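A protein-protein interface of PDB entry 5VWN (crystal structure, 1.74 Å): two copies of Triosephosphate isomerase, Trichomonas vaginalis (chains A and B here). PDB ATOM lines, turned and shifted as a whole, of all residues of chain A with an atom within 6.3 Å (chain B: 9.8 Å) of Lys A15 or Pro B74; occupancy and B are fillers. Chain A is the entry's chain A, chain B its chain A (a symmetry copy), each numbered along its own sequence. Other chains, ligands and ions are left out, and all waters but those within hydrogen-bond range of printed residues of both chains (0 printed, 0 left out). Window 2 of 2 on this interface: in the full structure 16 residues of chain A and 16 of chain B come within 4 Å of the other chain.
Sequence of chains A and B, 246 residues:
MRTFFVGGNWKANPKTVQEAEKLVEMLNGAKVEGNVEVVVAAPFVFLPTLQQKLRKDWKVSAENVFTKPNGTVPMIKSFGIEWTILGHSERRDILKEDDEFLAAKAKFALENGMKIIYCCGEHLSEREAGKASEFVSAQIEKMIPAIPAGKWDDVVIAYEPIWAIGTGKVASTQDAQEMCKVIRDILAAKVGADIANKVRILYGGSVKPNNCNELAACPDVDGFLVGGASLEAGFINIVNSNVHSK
Hydrophobic or aromatic side chains of chain B within 4 Å of the printed part of chain A: Pro B74, Met B75 and Phe B79.
Along chain B the printed residues that touch a printed residue of chain A span positions 74 to 79.
Among the printed residues, 10 pairs touch across the chains.
Among the printed residues, no Asp or Glu carboxylate lies within 4 Å of a Lys or Arg side-chain nitrogen of the other chain.
Lys A15 touches just these residues of chain B: Pro B74 and Met B75.
Of chain A, only Lys A15 (3.1 Å) comes within 4 Å of Pro B74.
Asn A13 touches just one residue of chain B: Met B75 (3.9 Å).
Of chain B, only Met B75 (3.6 Å) comes within 4 Å of Pro A14.
Of the printed residues of chain B, Phe A46 touches Met B75 (3.9 Å) and Phe B79 (3.98 Å).
Printed residues of chain A within 4 Å of Met B75: Ala A12, Asn A13, Pro A14, Lys A15 and Phe A46.
Of the printed residues of chain A, Ser B78 touches Thr A16 and Val A17.
The nearest residue of chain A that does not touch Pro B74 is Thr A16 (4.5 Å).
No position is printed for both chains.
Ala A12 touches Met B75.
Asn A13 touches Met B75.
Pro A14 touches Met B75.
Ser B78 touches Thr A16.
CZ of Phe B79 touches CG2 of Val A17 (3.6 Å).
CZ of Phe A46 touches CG of Met B75 (3.9 Å).
Phe B79 touches Phe A46 (CE2 to CE1, 3.98 Å).
The backbone NH (N) of Val A17 lies within hydrogen-bond range of the side-chain hydroxyl (OG) of Ser B78 (3.0 Å).
The backbone NH (N) of Met B75 sits at hydrogen-bond distance from the backbone carbonyl oxygen (O) of Lys A15 (3.1 Å).
The backbone carbonyl oxygen of Lys A15 lies close to the backbone carbonyl oxygen of Pro B74 (3.3 Å).
The side-chain hydroxyl of Thr A16 is in hydrogen-bond range of the side-chain carboxylate of Glu A19 (2.8 Å).
OG of Ser B78 sits at hydrogen-bond distance from O of Met B75, 2.7 Å away.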
ATOM      1  N   ALA A  12     -29.527  -0.880  -2.598  1.00  0.00           N
ATOM      2  CA  ALA A  12     -28.919  -1.100  -1.287  1.00  0.00           C
ATOM      3  C   ALA A  12     -27.396  -1.151  -1.400  1.00  0.00           C
ATOM      4  O   ALA A  12     -26.762  -2.169  -1.115  1.00  0.00           O
ATOM      5  CB  ALA A  12     -29.470  -2.380  -0.656  1.00  0.00           C
ATOM      6  N   ASN A  13     -26.815  -0.023  -1.817  1.00  0.00           N
ATOM      7  CA  ASN A  13     -25.384   0.111  -2.119  1.00  0.00           C
ATOM      8  C   ASN A  13     -24.957   1.560  -1.898  1.00  0.00           C
ATOM      9  O   ASN A  13     -25.805   2.466  -1.958  1.00  0.00           O
ATOM     10  CB  ASN A  13     -25.081  -0.270  -3.576  1.00  0.00           C
ATOM     11  CG  ASN A  13     -25.501  -1.681  -3.916  1.00  0.00           C
ATOM     12  OD1 ASN A  13     -24.776  -2.641  -3.635  1.00  0.00           O
ATOM     13  ND2 ASN A  13     -26.673  -1.820  -4.532  1.00  0.00           N
ATOM     14  N   PRO A  14     -23.658   1.800  -1.630  1.00  0.00           N
ATOM     15  CA  PRO A  14     -22.614   0.806  -1.342  1.00  0.00           C
ATOM     16  C   PRO A  14     -22.769   0.289   0.084  1.00  0.00           C
ATOM     17  O   PRO A  14     -23.725   0.650   0.756  1.00  0.00           O
ATOM     18  CB  PRO A  14     -21.316   1.594  -1.499  1.00  0.00           C
ATOM     19  CG  PRO A  14     -21.691   2.978  -1.141  1.00  0.00           C
ATOM     20  CD  PRO A  14     -23.131   3.174  -1.582  1.00  0.00           C
ATOM     21  N   LYS A  15     -21.852  -0.544   0.558  1.00  0.00           N
ATOM     22  CA  LYS A  15     -22.103  -1.158   1.855  1.00  0.00           C
ATOM     23  C   LYS A  15     -21.554  -0.349   3.028  1.00  0.00           C
ATOM     24  O   LYS A  15     -21.875  -0.680   4.174  1.00  0.00           O
ATOM     25  CB  LYS A  15     -21.543  -2.588   1.875  1.00  0.00           C
ATOM     26  CG  LYS A  15     -22.257  -3.520   0.891  1.00  0.00           C
ATOM     27  CD  LYS A  15     -23.786  -3.368   0.984  1.00  0.00           C
ATOM     28  CE  LYS A  15     -24.511  -4.222  -0.043  1.00  0.00           C
ATOM     29  N   THR A  16     -20.767   0.706   2.778  1.00  0.00           N
ATOM     30  CA  THR A  16     -20.211   1.555   3.831  1.00  0.00           C
ATOM     31  C   THR A  16     -20.310   3.033   3.472  1.00  0.00           C
ATOM     32  O   THR A  16     -20.277   3.414   2.294  1.00  0.00           O
ATOM     33  CB  THR A  16     -18.730   1.226   4.119  1.00  0.00           C
ATOM     34  OG1 THR A  16     -17.916   1.600   2.995  1.00  0.00           O
ATOM     35  CG2 THR A  16     -18.545  -0.262   4.370  1.00  0.00           C
ATOM     36  N   VAL A  17     -20.386   3.873   4.513  1.00  0.00           N
ATOM     37  CA  VAL A  17     -20.444   5.319   4.292  1.00  0.00           C
ATOM     38  C   VAL A  17     -19.134   5.824   3.708  1.00  0.00           C
ATOM     39  O   VAL A  17     -19.124   6.801   2.950  1.00  0.00           O
ATOM     40  CB  VAL A  17     -20.810   6.070   5.591  1.00  0.00           C
ATOM     41  CG1 VAL A  17     -19.667   6.006   6.608  1.00  0.00           C
ATOM     42  CG2 VAL A  17     -21.187   7.547   5.288  1.00  0.00           C
ATOM     43  N   GLU A  19     -17.345   4.260   1.454  1.00  0.00           N
ATOM     44  CA  GLU A  19     -17.496   4.042   0.010  1.00  0.00           C
ATOM     45  C   GLU A  19     -18.467   5.048  -0.609  1.00  0.00           C
ATOM     46  O   GLU A  19     -18.272   5.495  -1.754  1.00  0.00           O
ATOM     47  CB  GLU A  19     -17.992   2.628  -0.274  1.00  0.00           C
ATOM     48  CG  GLU A  19     -17.014   1.493  -0.020  1.00  0.00           C
ATOM     49  CD  GLU A  19     -17.714   0.147  -0.106  1.00  0.00           C
ATOM     50  OE1 GLU A  19     -18.305  -0.299   0.911  1.00  0.00           O
ATOM     51  OE2 GLU A  19     -17.710  -0.449  -1.203  1.00  0.00           O
ATOM     52  N   PHE A  46     -27.426   6.995   4.208  1.00  0.00           N
ATOM     53  CA  PHE A  46     -26.490   7.805   3.438  1.00  0.00           C
ATOM     54  C   PHE A  46     -27.075   9.124   2.938  1.00  0.00           C
ATOM     55  O   PHE A  46     -26.318   9.948   2.408  1.00  0.00           O
ATOM     56  CB  PHE A  46     -25.972   7.013   2.225  1.00  0.00           C
ATOM     57  CG  PHE A  46     -25.219   5.767   2.584  1.00  0.00           C
ATOM     58  CD1 PHE A  46     -24.608   5.633   3.828  1.00  0.00           C
ATOM     59  CD2 PHE A  46     -25.111   4.724   1.667  1.00  0.00           C
ATOM     60  CE1 PHE A  46     -23.892   4.465   4.162  1.00  0.00           C
ATOM     61  CE2 PHE A  46     -24.416   3.571   1.983  1.00  0.00           C
ATOM     62  CZ  PHE A  46     -23.813   3.433   3.236  1.00  0.00           C
ATOM     63  N   ASN B  64     -34.193  -1.579  13.056  1.00  0.00           N
ATOM     64  CA  ASN B  64     -34.369  -2.850  12.353  1.00  0.00           C
ATOM     65  C   ASN B  64     -33.157  -3.012  11.443  1.00  0.00           C
ATOM     66  O   ASN B  64     -32.411  -2.059  11.213  1.00  0.00           O
ATOM     67  CB  ASN B  64     -35.677  -2.873  11.552  1.00  0.00           C
ATOM     68  CG  ASN B  64     -36.079  -4.269  11.106  1.00  0.00           C
ATOM     69  OD1 ASN B  64     -35.483  -5.274  11.510  1.00  0.00           O
ATOM     70  ND2 ASN B  64     -37.111  -4.337  10.272  1.00  0.00           N
ATOM     71  N   VAL B  65     -32.954  -4.231  10.942  1.00  0.00           N
ATOM     72  CA  VAL B  65     -31.920  -4.455   9.921  1.00  0.00           C
ATOM     73  C   VAL B  65     -32.416  -5.471   8.897  1.00  0.00           C
ATOM     74  O   VAL B  65     -33.356  -6.222   9.161  1.00  0.00           O
ATOM     75  CB  VAL B  65     -30.569  -4.924  10.522  1.00  0.00           C
ATOM     76  CG1 VAL B  65     -29.889  -3.810  11.324  1.00  0.00           C
ATOM     77  CG2 VAL B  65     -30.749  -6.194  11.354  1.00  0.00           C
ATOM     78  N   VAL B  73     -26.682  -4.238   7.574  1.00  0.00           N
ATOM     79  CA  VAL B  73     -25.803  -4.276   8.756  1.00  0.00           C
ATOM     80  C   VAL B  73     -24.431  -3.627   8.520  1.00  0.00           C
ATOM     81  O   VAL B  73     -23.960  -2.861   9.364  1.00  0.00           O
ATOM     82  CB  VAL B  73     -25.640  -5.734   9.263  1.00  0.00           C
ATOM     83  CG1 VAL B  73     -24.414  -5.856  10.153  1.00  0.00           C
ATOM     84  CG2 VAL B  73     -26.885  -6.155  10.020  1.00  0.00           C
ATOM     85  N   PRO B  74     -23.767  -3.903   7.392  1.00  0.00           N
ATOM     86  CA  PRO B  74     -22.483  -3.218   7.161  1.00  0.00           C
ATOM     87  C   PRO B  74     -22.633  -1.706   7.045  1.00  0.00           C
ATOM     88  O   PRO B  74     -21.721  -0.966   7.439  1.00  0.00           O
ATOM     89  CB  PRO B  74     -21.967  -3.850   5.860  1.00  0.00           C
ATOM     90  CG  PRO B  74     -23.144  -4.474   5.226  1.00  0.00           C
ATOM     91  CD  PRO B  74     -24.023  -4.919   6.356  1.00  0.00           C
ATOM     92  N   MET B  75     -23.773  -1.226   6.542  1.00  0.00           N
ATOM     93  CA  MET B  75     -23.979   0.219   6.439  1.00  0.00           C
ATOM     94  C   MET B  75     -23.991   0.871   7.812  1.00  0.00           C
ATOM     95  O   MET B  75     -23.318   1.881   8.035  1.00  0.00           O
ATOM     96  CB  MET B  75     -25.292   0.525   5.708  1.00  0.00           C
ATOM     97  CG  MET B  75     -25.395  -0.019   4.306  1.00  0.00           C
ATOM     98  SD  MET B  75     -26.978   0.547   3.627  1.00  0.00           S
ATOM     99  CE  MET B  75     -26.974  -0.333   2.065  1.00  0.00           C
ATOM    100  N   ILE B  76     -24.786   0.335   8.748  1.00  0.00           N
ATOM    101  CA  ILE B  76     -24.823   1.007  10.048  1.00  0.00           C
ATOM    102  C   ILE B  76     -23.525   0.770  10.824  1.00  0.00           C
ATOM    103  O   ILE B  76     -23.057   1.674  11.526  1.00  0.00           O
ATOM    104  CB  ILE B  76     -26.057   0.593  10.876  1.00  0.00           C
ATOM    105  CG1 ILE B  76     -26.008  -0.881  11.244  1.00  0.00           C
ATOM    106  CG2 ILE B  76     -27.361   0.969  10.136  1.00  0.00           C
ATOM    107  CD1 ILE B  76     -27.149  -1.295  12.168  1.00  0.00           C
ATOM    108  N   LYS B  77     -22.901  -0.406  10.668  1.00  0.00           N
ATOM    109  CA  LYS B  77     -21.606  -0.651  11.307  1.00  0.00           C
ATOM    110  C   LYS B  77     -20.541   0.320  10.818  1.00  0.00           C
ATOM    111  O   LYS B  77     -19.625   0.663  11.577  1.00  0.00           O
ATOM    112  CB  LYS B  77     -21.147  -2.098  11.078  1.00  0.00           C
ATOM    113  CG  LYS B  77     -21.897  -3.134  11.909  1.00  0.00           C
ATOM    114  CD  LYS B  77     -21.266  -4.512  11.809  1.00  0.00           C
ATOM    115  CE  LYS B  77     -19.973  -4.545  12.606  1.00  0.00           C
ATOM    116  NZ  LYS B  77     -19.264  -5.843  12.443  1.00  0.00           N
ATOM    117  N   SER B  78     -20.657   0.806   9.578  1.00  0.00           N
ATOM    118  CA  SER B  78     -19.649   1.732   9.072  1.00  0.00           C
ATOM    119  C   SER B  78     -19.700   3.093   9.762  1.00  0.00           C
ATOM    120  O   SER B  78     -18.743   3.866   9.644  1.00  0.00           O
ATOM    121  CB  SER B  78     -19.781   1.881   7.550  1.00  0.00           C
ATOM    122  OG  SER B  78     -20.917   2.655   7.182  1.00  0.00           O
ATOM    123  N   PHE B  79     -20.780   3.398  10.491  1.00  0.00           N
ATOM    124  CA  PHE B  79     -20.867   4.583  11.327  1.00  0.00           C
ATOM    125  C   PHE B  79     -20.414   4.335  12.758  1.00  0.00           C
ATOM    126  O   PHE B  79     -20.348   5.291  13.536  1.00  0.00           O
ATOM    127  CB  PHE B  79     -22.305   5.099  11.381  1.00  0.00           C
ATOM    128  CG  PHE B  79     -22.784   5.699  10.095  1.00  0.00           C
ATOM    129  CD1 PHE B  79     -22.540   7.031   9.809  1.00  0.00           C
ATOM    130  CD2 PHE B  79     -23.499   4.936   9.187  1.00  0.00           C
ATOM    131  CE1 PHE B  79     -23.002   7.593   8.618  1.00  0.00           C
ATOM    132  CE2 PHE B  79     -23.952   5.489   8.009  1.00  0.00           C
ATOM    133  CZ  PHE B  79     -23.704   6.807   7.726  1.00  0.00           C
ATOM    134  N   GLY B  80     -20.121   3.094  13.114  1.00  0.00           N
ATOM    135  CA  GLY B  80     -19.800   2.748  14.487  1.00  0.00           C
ATOM    136  C   GLY B  80     -20.991   2.358  15.335  1.00  0.00           C
ATOM    137  O   GLY B  80     -20.850   2.256  16.561  1.00  0.00           O
ATOM    138  N   ILE B  81     -22.157   2.148  14.725  1.00  0.00           N
ATOM    139  CA  ILE B  81     -23.364   1.759  15.456  1.00  0.00           C
ATOM    140  C   ILE B  81     -23.295   0.268  15.783  1.00  0.00           C
ATOM    141  O   ILE B  81     -23.000  -0.563  14.914  1.00  0.00           O
ATOM    142  CB  ILE B  81     -24.620   2.124  14.643  1.00  0.00           C
ATOM    143  CG1 ILE B  81     -24.710   3.643  14.513  1.00  0.00           C
ATOM    144  CG2 ILE B  81     -25.893   1.525  15.282  1.00  0.00           C
ATOM    145  CD1 ILE B  81     -25.690   4.117  13.435  1.00  0.00           C
ATOM    146  N   PHE B 108     -27.960 -13.972  12.054  1.00  0.00           N
ATOM    147  CA  PHE B 108     -27.129 -13.200  11.135  1.00  0.00           C
ATOM    148  C   PHE B 108     -26.537 -11.970  11.816  1.00  0.00           C
ATOM    149  O   PHE B 108     -25.343 -11.684  11.681  1.00  0.00           O
ATOM    150  CB  PHE B 108     -27.933 -12.793   9.894  1.00  0.00           C
ATOM    151  CG  PHE B 108     -27.114 -12.020   8.883  1.00  0.00           C
ATOM    152  CD1 PHE B 108     -26.353 -12.686   7.935  1.00  0.00           C
ATOM    153  CD2 PHE B 108     -27.074 -10.632   8.906  1.00  0.00           C
ATOM    154  CE1 PHE B 108     -25.585 -11.988   7.021  1.00  0.00           C
ATOM    155  CE2 PHE B 108     -26.303  -9.930   7.994  1.00  0.00           C
ATOM    156  CZ  PHE B 108     -25.557 -10.610   7.052  1.00  0.00           C
ATOM    157  N   ALA B 109     -27.353 -11.235  12.575  1.00  0.00           N
ATOM    158  CA  ALA B 109     -26.866  -9.998  13.176  1.00  0.00           C
ATOM    159  C   ALA B 109     -25.764 -10.263  14.199  1.00  0.00           C
ATOM    160  O   ALA B 109     -24.750  -9.554  14.230  1.00  0.00           O
ATOM    161  CB  ALA B 109     -28.027  -9.237  13.819  1.00  0.00           C
ATOM    162  N   ASN B 112     -22.524 -11.189  12.697  1.00  0.00           N
ATOM    163  CA  ASN B 112     -21.857 -10.053  12.080  1.00  0.00           C
ATOM    164  C   ASN B 112     -21.495  -8.969  13.085  1.00  0.00           C
ATOM    165  O   ASN B 112     -21.221  -7.831  12.689  1.00  0.00           O
ATOM    166  CB  ASN B 112     -22.716  -9.482  10.958  1.00  0.00           C
ATOM    167  CG  ASN B 112     -22.592 -10.286   9.685  1.00  0.00           C
ATOM    168  OD1 ASN B 112     -21.743  -9.997   8.842  1.00  0.00           O
ATOM    169  ND2 ASN B 112     -23.420 -11.319   9.547  1.00  0.00           N
ATOM    170  N   GLY B 113     -21.488  -9.297  14.373  1.00  0.00           N
ATOM    171  CA  GLY B 113     -20.961  -8.409  15.381  1.00  0.00           C
ATOM    172  C   GLY B 113     -21.932  -7.410  15.976  1.00  0.00           C
ATOM    173  O   GLY B 113     -21.485  -6.489  16.666  1.00  0.00           O
ATOM    174  N   MET B 114     -23.231  -7.571  15.752  1.00  0.00           N
ATOM    175  CA  MET B 114     -24.232  -6.675  16.326  1.00  0.00           C
ATOM    176  C   MET B 114     -24.681  -7.186  17.692  1.00  0.00           C
ATOM    177  O   MET B 114     -24.641  -8.394  17.960  1.00  0.00           O
ATOM    178  CB  MET B 114     -25.449  -6.567  15.411  1.00  0.00           C
ATOM    179  CG  MET B 114     -25.133  -6.169  13.991  1.00  0.00           C
ATOM    180  SD  MET B 114     -24.724  -4.422  13.937  1.00  0.00           S
ATOM    181  CE  MET B 114     -26.239  -3.673  14.577  1.00  0.00           C
